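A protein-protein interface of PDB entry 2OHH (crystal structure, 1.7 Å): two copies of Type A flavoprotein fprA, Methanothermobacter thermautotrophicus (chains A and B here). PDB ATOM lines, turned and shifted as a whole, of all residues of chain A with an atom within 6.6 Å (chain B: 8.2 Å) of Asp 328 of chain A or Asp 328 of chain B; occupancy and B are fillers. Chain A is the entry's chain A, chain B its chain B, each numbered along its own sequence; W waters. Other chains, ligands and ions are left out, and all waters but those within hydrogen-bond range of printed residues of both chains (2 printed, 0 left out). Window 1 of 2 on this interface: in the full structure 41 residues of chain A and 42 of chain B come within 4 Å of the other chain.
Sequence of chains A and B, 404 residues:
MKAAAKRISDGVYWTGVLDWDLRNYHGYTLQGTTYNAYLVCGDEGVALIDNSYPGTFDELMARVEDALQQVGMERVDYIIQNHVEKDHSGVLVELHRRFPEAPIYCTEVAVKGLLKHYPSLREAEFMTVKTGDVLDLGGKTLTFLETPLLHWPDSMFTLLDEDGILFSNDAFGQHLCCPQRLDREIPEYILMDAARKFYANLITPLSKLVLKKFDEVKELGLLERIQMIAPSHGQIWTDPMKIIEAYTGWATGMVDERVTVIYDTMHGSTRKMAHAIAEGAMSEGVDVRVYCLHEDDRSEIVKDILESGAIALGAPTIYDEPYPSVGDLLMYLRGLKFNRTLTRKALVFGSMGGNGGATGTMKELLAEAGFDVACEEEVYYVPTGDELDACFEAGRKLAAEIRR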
ATOM      1  N   ARG A 298      -8.641 -24.222  12.937  1.00  0.00           N
ATOM      2  CA  ARG A 298      -7.307 -24.085  12.281  1.00  0.00           C
ATOM      3  C   ARG A 298      -7.056 -25.237  11.335  1.00  0.00           C
ATOM      4  O   ARG A 298      -6.441 -25.022  10.327  1.00  0.00           O
ATOM      5  CB  ARG A 298      -6.194 -24.062  13.311  1.00  0.00           C
ATOM      6  CG  ARG A 298      -6.056 -25.335  14.092  1.00  0.00           C
ATOM      7  CD  ARG A 298      -4.870 -25.195  15.086  1.00  0.00           C
ATOM      8  NE  ARG A 298      -5.265 -24.663  16.390  1.00  0.00           N
ATOM      9  CZ  ARG A 298      -5.747 -25.402  17.387  1.00  0.00           C
ATOM     10  NH1 ARG A 298      -6.012 -26.691  17.233  1.00  0.00           N
ATOM     11  NH2 ARG A 298      -6.020 -24.824  18.549  1.00  0.00           N
ATOM     12  N   TYR A 323      -6.008  -9.367  17.544  1.00  0.00           N
ATOM     13  CA  TYR A 323      -6.991 -10.159  18.224  1.00  0.00           C
ATOM     14  C   TYR A 323      -6.390 -11.564  18.429  1.00  0.00           C
ATOM     15  O   TYR A 323      -5.871 -12.166  17.492  1.00  0.00           O
ATOM     16  CB  TYR A 323      -8.253 -10.164  17.396  1.00  0.00           C
ATOM     17  CG  TYR A 323      -9.340 -10.811  18.165  1.00  0.00           C
ATOM     18  CD1 TYR A 323     -10.000 -10.107  19.180  1.00  0.00           C
ATOM     19  CD2 TYR A 323      -9.628 -12.130  17.956  1.00  0.00           C
ATOM     20  CE1 TYR A 323     -10.997 -10.712  19.932  1.00  0.00           C
ATOM     21  CE2 TYR A 323     -10.577 -12.753  18.699  1.00  0.00           C
ATOM     22  CZ  TYR A 323     -11.242 -12.051  19.706  1.00  0.00           C
ATOM     23  OH  TYR A 323     -12.207 -12.699  20.430  1.00  0.00           O
ATOM     24  N   PRO A 324      -6.442 -12.080  19.666  1.00  0.00           N
ATOM     25  CA  PRO A 324      -5.579 -13.169  20.007  1.00  0.00           C
ATOM     26  C   PRO A 324      -5.827 -14.473  19.281  1.00  0.00           C
ATOM     27  O   PRO A 324      -4.947 -15.366  19.282  1.00  0.00           O
ATOM     28  CB  PRO A 324      -5.756 -13.296  21.533  1.00  0.00           C
ATOM     29  CG  PRO A 324      -7.100 -12.855  21.774  1.00  0.00           C
ATOM     30  CD  PRO A 324      -7.222 -11.649  20.840  1.00  0.00           C
ATOM     31  N   SER A 325      -7.005 -14.614  18.690  1.00  0.00           N
ATOM     32  CA  SER A 325      -7.283 -15.868  17.950  1.00  0.00           C
ATOM     33  C   SER A 325      -6.294 -16.056  16.830  1.00  0.00           C
ATOM     34  O   SER A 325      -5.976 -17.210  16.485  1.00  0.00           O
ATOM     35  CB  SER A 325      -8.683 -15.861  17.364  1.00  0.00           C
ATOM     36  OG  SER A 325      -8.803 -14.800  16.441  1.00  0.00           O
ATOM     37  N   VAL A 326      -5.726 -14.986  16.275  1.00  0.00           N
ATOM     38  CA  VAL A 326      -4.751 -15.203  15.187  1.00  0.00           C
ATOM     39  C   VAL A 326      -3.481 -15.766  15.766  1.00  0.00           C
ATOM     40  O   VAL A 326      -2.728 -16.370  15.044  1.00  0.00           O
ATOM     41  CB  VAL A 326      -4.430 -13.971  14.322  1.00  0.00           C
ATOM     42  CG1 VAL A 326      -5.738 -13.414  13.749  1.00  0.00           C
ATOM     43  CG2 VAL A 326      -3.784 -12.988  15.151  1.00  0.00           C
ATOM     44  N   GLY A 327      -3.283 -15.605  17.074  1.00  0.00           N
ATOM     45  CA  GLY A 327      -2.108 -16.162  17.724  1.00  0.00           C
ATOM     46  C   GLY A 327      -2.064 -17.662  17.630  1.00  0.00           C
ATOM     47  O   GLY A 327      -1.008 -18.237  17.570  1.00  0.00           O
ATOM     48  N   ASP A 328      -3.231 -18.273  17.694  1.00  0.00           N
ATOM     49  CA  ASP A 328      -3.302 -19.711  17.661  1.00  0.00           C
ATOM     50  C   ASP A 328      -2.936 -20.146  16.244  1.00  0.00           C
ATOM     51  O   ASP A 328      -2.057 -20.992  16.036  1.00  0.00           O
ATOM     52  CB  ASP A 328      -4.709 -20.121  18.099  1.00  0.00           C
ATOM     53  CG  ASP A 328      -4.950 -21.617  17.929  1.00  0.00           C
ATOM     54  OD1 ASP A 328      -4.710 -22.113  16.812  1.00  0.00           O
ATOM     55  OD2 ASP A 328      -5.445 -22.300  18.872  1.00  0.00           O
ATOM     56  N   LEU A 329      -3.596 -19.537  15.254  1.00  0.00           N
ATOM     57  CA  LEU A 329      -3.337 -19.937  13.873  1.00  0.00           C
ATOM     58  C   LEU A 329      -1.901 -19.652  13.550  1.00  0.00           C
ATOM     59  O   LEU A 329      -1.244 -20.484  12.937  1.00  0.00           O
ATOM     60  CB  LEU A 329      -4.220 -19.158  12.937  1.00  0.00           C
ATOM     61  CG  LEU A 329      -4.045 -19.523  11.450  1.00  0.00           C
ATOM     62  CD1 LEU A 329      -4.384 -20.957  11.219  1.00  0.00           C
ATOM     63  CD2 LEU A 329      -4.945 -18.572  10.660  1.00  0.00           C
ATOM     64  N   LEU A 330      -1.402 -18.491  13.984  1.00  0.00           N
ATOM     65  CA  LEU A 330      -0.066 -18.199  13.579  1.00  0.00           C
ATOM     66  C   LEU A 330       0.980 -19.144  14.199  1.00  0.00           C
ATOM     67  O   LEU A 330       2.034 -19.397  13.591  1.00  0.00           O
ATOM     68  CB  LEU A 330       0.277 -16.741  13.855  1.00  0.00           C
ATOM     69  CG  LEU A 330      -0.430 -15.794  12.864  1.00  0.00           C
ATOM     70  CD1 LEU A 330      -0.247 -14.369  13.427  1.00  0.00           C
ATOM     71  CD2 LEU A 330       0.349 -15.857  11.514  1.00  0.00           C
ATOM     72  N   MET A 331       0.712 -19.607  15.413  1.00  0.00           N
ATOM     73  CA  MET A 331       1.644 -20.510  16.094  1.00  0.00           C
ATOM     74  C   MET A 331       1.574 -21.817  15.365  1.00  0.00           C
ATOM     75  O   MET A 331       2.564 -22.509  15.201  1.00  0.00           O
ATOM     76  CB  MET A 331       1.310 -20.685  17.585  1.00  0.00           C
ATOM     77  CG  MET A 331       2.397 -21.449  18.335  1.00  0.00           C
ATOM     78  SD  MET A 331       2.217 -21.203  20.086  1.00  0.00           S
ATOM     79  CE  MET A 331       2.978 -19.605  20.340  1.00  0.00           C
ATOM     80  N   TYR A 332       0.360 -22.173  14.968  1.00  0.00           N
ATOM     81  CA  TYR A 332       0.161 -23.425  14.217  1.00  0.00           C
ATOM     82  C   TYR A 332       0.899 -23.348  12.882  1.00  0.00           C
ATOM     83  O   TYR A 332       1.663 -24.247  12.526  1.00  0.00           O
ATOM     84  CB  TYR A 332      -1.316 -23.590  13.977  1.00  0.00           C
ATOM     85  CG  TYR A 332      -1.674 -24.999  13.569  1.00  0.00           C
ATOM     86  CD1 TYR A 332      -1.143 -26.086  14.241  1.00  0.00           C
ATOM     87  CD2 TYR A 332      -2.577 -25.225  12.527  1.00  0.00           C
ATOM     88  CE1 TYR A 332      -1.557 -27.403  13.892  1.00  0.00           C
ATOM     89  CE2 TYR A 332      -2.953 -26.517  12.182  1.00  0.00           C
ATOM     90  CZ  TYR A 332      -2.438 -27.563  12.859  1.00  0.00           C
ATOM     91  OH  TYR A 332      -2.778 -28.845  12.544  1.00  0.00           O
ATOM     92  N   LEU A 333       0.738 -22.228  12.192  1.00  0.00           N
ATOM     93  CA  LEU A 333       1.453 -22.033  10.934  1.00  0.00           C
ATOM     94  C   LEU A 333       2.947 -22.047  11.140  1.00  0.00           C
ATOM     95  O   LEU A 333       3.681 -22.522  10.284  1.00  0.00           O
ATOM     96  CB  LEU A 333       1.040 -20.749  10.247  1.00  0.00           C
ATOM     97  CG  LEU A 333      -0.423 -20.796   9.776  1.00  0.00           C
ATOM     98  CD1 LEU A 333      -0.766 -19.384   9.339  1.00  0.00           C
ATOM     99  CD2 LEU A 333      -0.662 -21.758   8.626  1.00  0.00           C
ATOM    100  N   GLY B  27     -14.050 -11.506  22.419  1.00  0.00           N
ATOM    101  CA  GLY B  27     -13.339 -12.594  23.059  1.00  0.00           C
ATOM    102  C   GLY B  27     -13.343 -12.585  24.572  1.00  0.00           C
ATOM    103  O   GLY B  27     -12.421 -13.144  25.181  1.00  0.00           O
ATOM    104  N   ASP B 264      -2.429 -27.120  27.898  1.00  0.00           N
ATOM    105  CA  ASP B 264      -3.109 -27.867  26.866  1.00  0.00           C
ATOM    106  C   ASP B 264      -2.389 -29.160  26.642  1.00  0.00           C
ATOM    107  O   ASP B 264      -1.287 -29.388  27.174  1.00  0.00           O
ATOM    108  CB  ASP B 264      -3.322 -27.028  25.579  1.00  0.00           C
ATOM    109  CG  ASP B 264      -4.674 -27.375  24.890  1.00  0.00           C
ATOM    110  OD1 ASP B 264      -5.210 -28.455  25.126  1.00  0.00           O
ATOM    111  OD2 ASP B 264      -5.168 -26.538  24.116  1.00  0.00           O
ATOM    112  N   LEU B 293      -6.641 -25.127  28.091  1.00  0.00           N
ATOM    113  CA  LEU B 293      -6.882 -24.247  26.956  1.00  0.00           C
ATOM    114  C   LEU B 293      -7.895 -24.810  25.932  1.00  0.00           C
ATOM    115  O   LEU B 293      -8.460 -24.065  25.157  1.00  0.00           O
ATOM    116  CB  LEU B 293      -5.559 -23.866  26.296  1.00  0.00           C
ATOM    117  CG  LEU B 293      -4.766 -22.912  27.177  1.00  0.00           C
ATOM    118  CD1 LEU B 293      -3.366 -22.764  26.548  1.00  0.00           C
ATOM    119  CD2 LEU B 293      -5.489 -21.519  27.334  1.00  0.00           C
ATOM    120  N   ASP B 296     -11.302 -23.873  28.184  1.00  0.00           N
ATOM    121  CA  ASP B 296     -11.535 -22.706  29.027  1.00  0.00           C
ATOM    122  C   ASP B 296     -11.251 -21.426  28.277  1.00  0.00           C
ATOM    123  O   ASP B 296     -10.359 -21.410  27.428  1.00  0.00           O
ATOM    124  CB  ASP B 296     -10.686 -22.817  30.255  1.00  0.00           C
ATOM    125  CG  ASP B 296     -11.119 -23.965  31.127  1.00  0.00           C
ATOM    126  OD1 ASP B 296     -12.341 -24.210  31.197  1.00  0.00           O
ATOM    127  OD2 ASP B 296     -10.253 -24.670  31.662  1.00  0.00           O
ATOM    128  N   ASP B 297     -12.013 -20.367  28.567  1.00  0.00           N
ATOM    129  CA  ASP B 297     -11.883 -19.136  27.796  1.00  0.00           C
ATOM    130  C   ASP B 297     -10.734 -18.351  28.310  1.00  0.00           C
ATOM    131  O   ASP B 297     -10.468 -18.278  29.496  1.00  0.00           O
ATOM    132  CB  ASP B 297     -13.136 -18.224  27.856  1.00  0.00           C
ATOM    133  CG  ASP B 297     -13.147 -17.186  26.708  1.00  0.00           C
ATOM    134  OD1 ASP B 297     -13.454 -17.584  25.542  1.00  0.00           O
ATOM    135  OD2 ASP B 297     -12.818 -15.970  26.936  1.00  0.00           O
ATOM    136  N   ARG B 298     -10.030 -17.725  27.394  1.00  0.00           N
ATOM    137  CA  ARG B 298      -8.944 -16.908  27.830  1.00  0.00           C
ATOM    138  C   ARG B 298      -9.398 -15.832  28.832  1.00  0.00           C
ATOM    139  O   ARG B 298      -8.637 -15.433  29.742  1.00  0.00           O
ATOM    140  CB  ARG B 298      -8.327 -16.220  26.625  1.00  0.00           C
ATOM    141  CG  ARG B 298      -9.181 -15.045  26.011  1.00  0.00           C
ATOM    142  CD  ARG B 298      -8.475 -14.503  24.800  1.00  0.00           C
ATOM    143  NE  ARG B 298      -8.511 -15.337  23.596  1.00  0.00           N
ATOM    144  CZ  ARG B 298      -9.530 -15.290  22.739  1.00  0.00           C
ATOM    145  NH1 ARG B 298     -10.582 -14.486  23.013  1.00  0.00           N
ATOM    146  NH2 ARG B 298      -9.539 -16.051  21.645  1.00  0.00           N
ATOM    147  N   SER B 299     -10.634 -15.377  28.683  1.00  0.00           N
ATOM    148  CA  SER B 299     -11.144 -14.272  29.571  1.00  0.00           C
ATOM    149  C   SER B 299     -11.266 -14.735  31.010  1.00  0.00           C
ATOM    150  O   SER B 299     -11.072 -13.957  31.934  1.00  0.00           O
ATOM    151  CB  SER B 299     -12.436 -13.641  29.018  1.00  0.00           C
ATOM    152  OG  SER B 299     -13.525 -14.576  28.955  1.00  0.00           O
ATOM    153  N   ILE B 301      -9.383 -17.287  32.247  1.00  0.00           N
ATOM    154  CA  ILE B 301      -8.041 -17.616  32.682  1.00  0.00           C
ATOM    155  C   ILE B 301      -7.430 -16.333  33.174  1.00  0.00           C
ATOM    156  O   ILE B 301      -6.821 -16.334  34.245  1.00  0.00           O
ATOM    157  CB  ILE B 301      -7.243 -18.217  31.531  1.00  0.00           C
ATOM    158  CG1 ILE B 301      -7.800 -19.601  31.196  1.00  0.00           C
ATOM    159  CG2 ILE B 301      -5.734 -18.214  31.778  1.00  0.00           C
ATOM    160  CD1 ILE B 301      -7.227 -20.129  29.884  1.00  0.00           C
ATOM    161  N   VAL B 302      -7.576 -15.241  32.432  1.00  0.00           N
ATOM    162  CA  VAL B 302      -6.854 -14.065  32.877  1.00  0.00           C
ATOM    163  C   VAL B 302      -7.484 -13.423  34.106  1.00  0.00           C
ATOM    164  O   VAL B 302      -6.809 -12.702  34.831  1.00  0.00           O
ATOM    165  CB  VAL B 302      -6.528 -13.016  31.768  1.00  0.00           C
ATOM    166  CG1 VAL B 302      -5.789 -13.652  30.646  1.00  0.00           C
ATOM    167  CG2 VAL B 302      -7.766 -12.334  31.307  1.00  0.00           C
ATOM    168  N   PRO B 322       4.939 -24.834  20.665  1.00  0.00           N
ATOM    169  CA  PRO B 322       3.891 -25.147  21.617  1.00  0.00           C
ATOM    170  C   PRO B 322       2.642 -25.495  20.854  1.00  0.00           C
ATOM    171  O   PRO B 322       2.393 -24.978  19.768  1.00  0.00           O
ATOM    172  CB  PRO B 322       3.647 -23.837  22.320  1.00  0.00           C
ATOM    173  CG  PRO B 322       4.904 -23.042  22.152  1.00  0.00           C
ATOM    174  CD  PRO B 322       5.311 -23.416  20.736  1.00  0.00           C
ATOM    175  N   TYR B 323       1.834 -26.316  21.476  1.00  0.00           N
ATOM    176  CA  TYR B 323       0.542 -26.619  20.981  1.00  0.00           C
ATOM    177  C   TYR B 323      -0.150 -25.246  20.785  1.00  0.00           C
ATOM    178  O   TYR B 323      -0.004 -24.338  21.624  1.00  0.00           O
ATOM    179  CB  TYR B 323      -0.191 -27.466  22.015  1.00  0.00           C
ATOM    180  CG  TYR B 323      -1.486 -27.877  21.475  1.00  0.00           C
ATOM    181  CD1 TYR B 323      -1.568 -28.956  20.615  1.00  0.00           C
ATOM    182  CD2 TYR B 323      -2.626 -27.153  21.749  1.00  0.00           C
ATOM    183  CE1 TYR B 323      -2.756 -29.299  20.043  1.00  0.00           C
ATOM    184  CE2 TYR B 323      -3.792 -27.481  21.212  1.00  0.00           C
ATOM    185  CZ  TYR B 323      -3.868 -28.573  20.359  1.00  0.00           C
ATOM    186  OH  TYR B 323      -5.078 -28.939  19.807  1.00  0.00           O
ATOM    187  N   PRO B 324      -0.830 -25.076  19.645  1.00  0.00           N
ATOM    188  CA  PRO B 324      -1.097 -23.707  19.209  1.00  0.00           C
ATOM    189  C   PRO B 324      -2.044 -22.878  20.021  1.00  0.00           C
ATOM    190  O   PRO B 324      -1.994 -21.654  19.927  1.00  0.00           O
ATOM    191  CB  PRO B 324      -1.522 -23.881  17.746  1.00  0.00           C
ATOM    192  CG  PRO B 324      -2.105 -25.275  17.709  1.00  0.00           C
ATOM    193  CD  PRO B 324      -1.196 -26.046  18.613  1.00  0.00           C
ATOM    194  N   SER B 325      -2.919 -23.534  20.785  1.00  0.00           N
ATOM    195  CA  SER B 325      -3.821 -22.803  21.688  1.00  0.00           C
ATOM    196  C   SER B 325      -3.042 -21.840  22.591  1.00  0.00           C
ATOM    197  O   SER B 325      -3.525 -20.739  22.904  1.00  0.00           O
ATOM    198  CB  SER B 325      -4.658 -23.819  22.484  1.00  0.00           C
ATOM    199  OG  SER B 325      -3.755 -24.536  23.301  1.00  0.00           O
ATOM    200  N   VAL B 326      -1.813 -22.219  22.967  1.00  0.00           N
ATOM    201  CA  VAL B 326      -1.058 -21.325  23.819  1.00  0.00           C
ATOM    202  C   VAL B 326      -0.692 -20.058  23.078  1.00  0.00           C
ATOM    203  O   VAL B 326      -0.513 -19.046  23.732  1.00  0.00           O
ATOM    204  CB  VAL B 326       0.221 -21.929  24.439  1.00  0.00           C
ATOM    205  CG1 VAL B 326      -0.039 -23.278  24.966  1.00  0.00           C
ATOM    206  CG2 VAL B 326       1.279 -21.967  23.496  1.00  0.00           C
ATOM    207  N   GLY B 327      -0.643 -20.088  21.746  1.00  0.00           N
ATOM    208  CA  GLY B 327      -0.352 -18.882  20.965  1.00  0.00           C
ATOM    209  C   GLY B 327      -1.445 -17.853  21.140  1.00  0.00           C
ATOM    210  O   GLY B 327      -1.194 -16.671  21.136  1.00  0.00           O
ATOM    211  N   ASP B 328      -2.665 -18.317  21.386  1.00  0.00           N
ATOM    212  CA  ASP B 328      -3.779 -17.391  21.545  1.00  0.00           C
ATOM    213  C   ASP B 328      -3.615 -16.729  22.916  1.00  0.00           C
ATOM    214  O   ASP B 328      -3.610 -15.507  23.035  1.00  0.00           O
ATOM    215  CB  ASP B 328      -5.096 -18.186  21.443  1.00  0.00           C
ATOM    216  CG  ASP B 328      -6.313 -17.370  21.788  1.00  0.00           C
ATOM    217  OD1 ASP B 328      -6.328 -16.716  22.873  1.00  0.00           O
ATOM    218  OD2 ASP B 328      -7.281 -17.381  20.986  1.00  0.00           O
ATOM    219  N   LEU B 329      -3.442 -17.540  23.942  1.00  0.00           N
ATOM    220  CA  LEU B 329      -3.383 -17.039  25.304  1.00  0.00           C
ATOM    221  C   LEU B 329      -2.167 -16.148  25.404  1.00  0.00           C
ATOM    222  O   LEU B 329      -2.221 -15.111  25.983  1.00  0.00           O
ATOM    223  CB  LEU B 329      -3.283 -18.163  26.319  1.00  0.00           C
ATOM    224  CG  LEU B 329      -3.110 -17.676  27.772  1.00  0.00           C
ATOM    225  CD1 LEU B 329      -4.324 -16.881  28.225  1.00  0.00           C
ATOM    226  CD2 LEU B 329      -2.964 -18.899  28.615  1.00  0.00           C
ATOM    227  N   LEU B 330      -1.055 -16.541  24.804  1.00  0.00           N
ATOM    228  CA  LEU B 330       0.114 -15.670  24.896  1.00  0.00           C
ATOM    229  C   LEU B 330      -0.037 -14.327  24.213  1.00  0.00           C
ATOM    230  O   LEU B 330       0.411 -13.296  24.726  1.00  0.00           O
ATOM    231  CB  LEU B 330       1.376 -16.379  24.409  1.00  0.00           C
ATOM    232  CG  LEU B 330       1.769 -17.542  25.348  1.00  0.00           C
ATOM    233  CD1 LEU B 330       2.770 -18.443  24.656  1.00  0.00           C
ATOM    234  CD2 LEU B 330       2.306 -17.072  26.657  1.00  0.00           C
ATOM    235  N   MET B 331      -0.652 -14.335  23.045  1.00  0.00           N
ATOM    236  CA  MET B 331      -0.873 -13.105  22.316  1.00  0.00           C
ATOM    237  C   MET B 331      -1.793 -12.219  23.127  1.00  0.00           C
ATOM    238  O   MET B 331      -1.573 -11.030  23.211  1.00  0.00           O
ATOM    239  CB  MET B 331      -1.457 -13.406  20.967  1.00  0.00           C
ATOM    240  CG  MET B 331      -1.739 -12.153  20.104  1.00  0.00           C
ATOM    241  SD  MET B 331      -2.018 -12.574  18.415  1.00  0.00           S
ATOM    242  CE  MET B 331      -0.312 -12.919  17.851  1.00  0.00           C
ATOM    243  N   TYR B 332      -2.786 -12.819  23.760  1.00  0.00           N
ATOM    244  CA  TYR B 332      -3.635 -12.067  24.693  1.00  0.00           C
ATOM    245  C   TYR B 332      -2.866 -11.507  25.879  1.00  0.00           C
ATOM    246  O   TYR B 332      -2.987 -10.294  26.205  1.00  0.00           O
ATOM    247  CB  TYR B 332      -4.773 -12.987  25.123  1.00  0.00           C
ATOM    248  CG  TYR B 332      -5.960 -12.282  25.691  1.00  0.00           C
ATOM    249  CD1 TYR B 332      -6.560 -11.230  24.988  1.00  0.00           C
ATOM    250  CD2 TYR B 332      -6.531 -12.711  26.901  1.00  0.00           C
ATOM    251  CE1 TYR B 332      -7.698 -10.602  25.490  1.00  0.00           C
ATOM    252  CE2 TYR B 332      -7.637 -12.089  27.409  1.00  0.00           C
ATOM    253  CZ  TYR B 332      -8.212 -11.035  26.679  1.00  0.00           C
ATOM    254  OH  TYR B 332      -9.339 -10.387  27.151  1.00  0.00           O
ATOM    255  N   LEU B 333      -2.026 -12.344  26.499  1.00  0.00           N
ATOM    256  CA  LEU B 333      -1.258 -11.923  27.660  1.00  0.00           C
ATOM    257  C   LEU B 333      -0.334 -10.818  27.291  1.00  0.00           C
ATOM    258  O   LEU B 333      -0.105  -9.890  28.079  1.00  0.00           O
ATOM    259  CB  LEU B 333      -0.448 -13.073  28.192  1.00  0.00           C
ATOM    260  CG  LEU B 333      -1.373 -14.008  28.961  1.00  0.00           C
ATOM    261  CD1 LEU B 333      -0.517 -15.181  29.499  1.00  0.00           C
ATOM    262  CD2 LEU B 333      -2.065 -13.278  30.054  1.00  0.00           C
ATOM    263  N   ARG B 334       0.125 -10.877  26.064  1.00  0.00           N
ATOM    264  CA  ARG B 334       1.035  -9.833  25.575  1.00  0.00           C
ATOM    265  C   ARG B 334       0.330  -8.492  25.520  1.00  0.00           C
ATOM    266  O   ARG B 334       0.912  -7.463  25.825  1.00  0.00           O
ATOM    267  CB  ARG B 334       1.534 -10.156  24.185  1.00  0.00           C
ATOM    268  CG  ARG B 334       2.975 -10.606  24.159  1.00  0.00           C
ATOM    269  CD  ARG B 334       3.466 -10.829  22.727  1.00  0.00           C
ATOM    270  NE  ARG B 334       3.693  -9.538  22.112  1.00  0.00           N
ATOM    271  CZ  ARG B 334       4.882  -8.971  21.904  1.00  0.00           C
ATOM    272  NH1 ARG B 334       6.021  -9.590  22.230  1.00  0.00           N
ATOM    273  NH2 ARG B 334       4.923  -7.771  21.341  1.00  0.00           N
ATOM    274  N   GLY B 335      -0.933  -8.485  25.147  1.00  0.00           N
ATOM    275  CA  GLY B 335      -1.694  -7.222  25.146  1.00  0.00           C
ATOM    276  C   GLY B 335      -2.000  -6.789  26.570  1.00  0.00           C
ATOM    277  O   GLY B 335      -2.024  -5.601  26.854  1.00  0.00           O
ATOM    278  N   LEU B 365       8.044 -16.408  25.485  1.00  0.00           N
ATOM    279  CA  LEU B 365       6.878 -15.619  25.226  1.00  0.00           C
ATOM    280  C   LEU B 365       6.241 -15.115  26.507  1.00  0.00           C
ATOM    281  O   LEU B 365       5.652 -14.031  26.539  1.00  0.00           O
ATOM    282  CB  LEU B 365       5.880 -16.453  24.425  1.00  0.00           C
ATOM    283  CG  LEU B 365       5.915 -16.439  22.899  1.00  0.00           C
ATOM    284  CD1 LEU B 365       7.306 -16.341  22.260  1.00  0.00           C
ATOM    285  CD2 LEU B 365       5.127 -17.699  22.401  1.00  0.00           C
HETATM  286  O   HOH W   1     -12.125 -15.388  20.257  1.00  0.00           O
HETATM  287  O   HOH W   2       1.746 -24.874  17.070  1.00  0.00           O
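Printed residues of chain A that touch a printed residue of chain B: Arg 298, Tyr 323, Pro 324, Ser 325, Val 326, Gly 327, Asp 328, Met 331 and Tyr 332. Printed residues of chain B that touch a printed residue of chain A: Gly 27, Arg 298, Pro 322, Tyr 323, Pro 324, Ser 325, Val 326, Gly 327, Asp 328, Met 331, Tyr 332 and Leu 365. Hydrophobic or aromatic side chains of chain B that line the printed part of chain A: Pro 322, Tyr 323, Pro 324, Val 326, Met 331, Tyr 332 and Leu 365. Among the printed residues, no Asp or Glu carboxylate lies within 4 Å of a Lys or Arg side-chain nitrogen of the other chain.
OH of Tyr 323 of chain A sits close to N of Gly 27 of chain B (3.0 Å). The side-chain sulfur (SD) of Met 331 of chain B is in hydrogen-bond range of the backbone NH (N) of Gly 327 of chain A (3.5 Å). The backbone NH of Ser 325 of chain B lies close to the side-chain carboxylate of Asp 328 of chain A (3.4 Å). N of Gly 327 of chain B lies within hydrogen-bond range of SD of Met 331 of chain A, 3.5 Å away. The side-chain sulfur (SD) of Met 331 of chain A lies close to the backbone carbonyl oxygen (O) of Pro 322 of chain B (3.8 Å).
Gly 327 of chain A touches just these residues of chain B: Gly 327, Asp 328 and Met 331. Of chain B, only Pro 324 (3.3 Å), Ser 325 (3.3 Å), Gly 327 (3.9 Å) and Asp 328 (3.7 Å) come within 4 Å of Asp 328 of chain A. Of the printed residues of chain A, Gly 27 of chain B touches Tyr 323. Printed residues of chain A within 4 Å of Tyr 323 of chain B: Arg 298. Printed residues of chain A within 4 Å of Val 326 of chain B: Met 331 (3.6 Å). Of chain A, only Pro 324 (3.3 Å), Ser 325 (3.4 Å), Gly 327 (3.9 Å) and Asp 328 (3.7 Å) come within 4 Å of Asp 328 of chain B. Printed residues of chain A within 4 Å of Tyr 332 of chain B: Pro 324. Leu 333 of chain B touches none of the printed residues of chain A. Gly 335 of chain B touches none of the printed residues of chain A. The nearest residue of chain A that does not touch Asp 328 of chain B is Val 326 of chain A (5.5 Å). The nearest printed residue of chain B that does not touch Ser 325 of chain A is Arg 298 of chain B (4.1 Å).
The guanidinium group of Arg 298 of chain A is in salt-bridge range of the side-chain carboxylate of Asp 328 of chain A. NH1 of Arg 298 of chain B lies within hydrogen-bond range of O of Gly 27 of chain B, 3.1 Å away. The side-chain carboxylate (OD2) of Asp 264 of chain B sits at hydrogen-bond distance from the side-chain hydroxyl (OG) of Ser 325 of chain B. OD1 of Asp 328 of chain B is in salt-bridge range of NE of Arg 298 of chain B, 2.7 Å away.
Ser 325 of chain A touches Asp 328 of chain B, and with the chains exchanged Asp 328 of chain A touches Ser 325 of chain B. Val 326 of chain A touches Met 331 of chain B, and with the chains exchanged Met 331 of chain A touches Val 326 of chain B. Gly 327 of chain B touches its own counterpart, Gly 327 of chain A. Asp 328 of chain A touches its own counterpart, Asp 328 of chain B. Positions printed for both chains: 298, 323, 324, 325, 326, 327, 328, 329, 330, 331, 332 and 333.
Tyr 323 of chain A touches Arg 298 of chain B. Pro 324 of chain A touches Arg 298 of chain B (CG to NE, 3.4 Å). Met 331 of chain B touches Pro 324 of chain A. CD1 of Tyr 332 of chain B touches CG of Pro 324 of chain A (3.6 Å). Asp 328 of chain B touches Ser 325 of chain A. CA of Asp 328 of chain A touches O of Pro 324 of chain B, 3.3 Å away. N of Asp 328 of chain A touches C of Gly 327 of chain B, at 3.9 Å. CD2 of Leu 365 of chain B touches CE of Met 331 of chain A (3.5 Å).
Water W1 lies within hydrogen-bond range of the side-chain hydroxyl (OH) of Tyr 323 of chain A (2.7 Å) and the guanidinium group (NH2) of Arg 298 of chain B (3.0 Å). Water W2 lies within hydrogen-bond range of the backbone carbonyl oxygen of Pro 322 of chain B and the backbone carbonyl oxygen of Met 331 of chain A.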
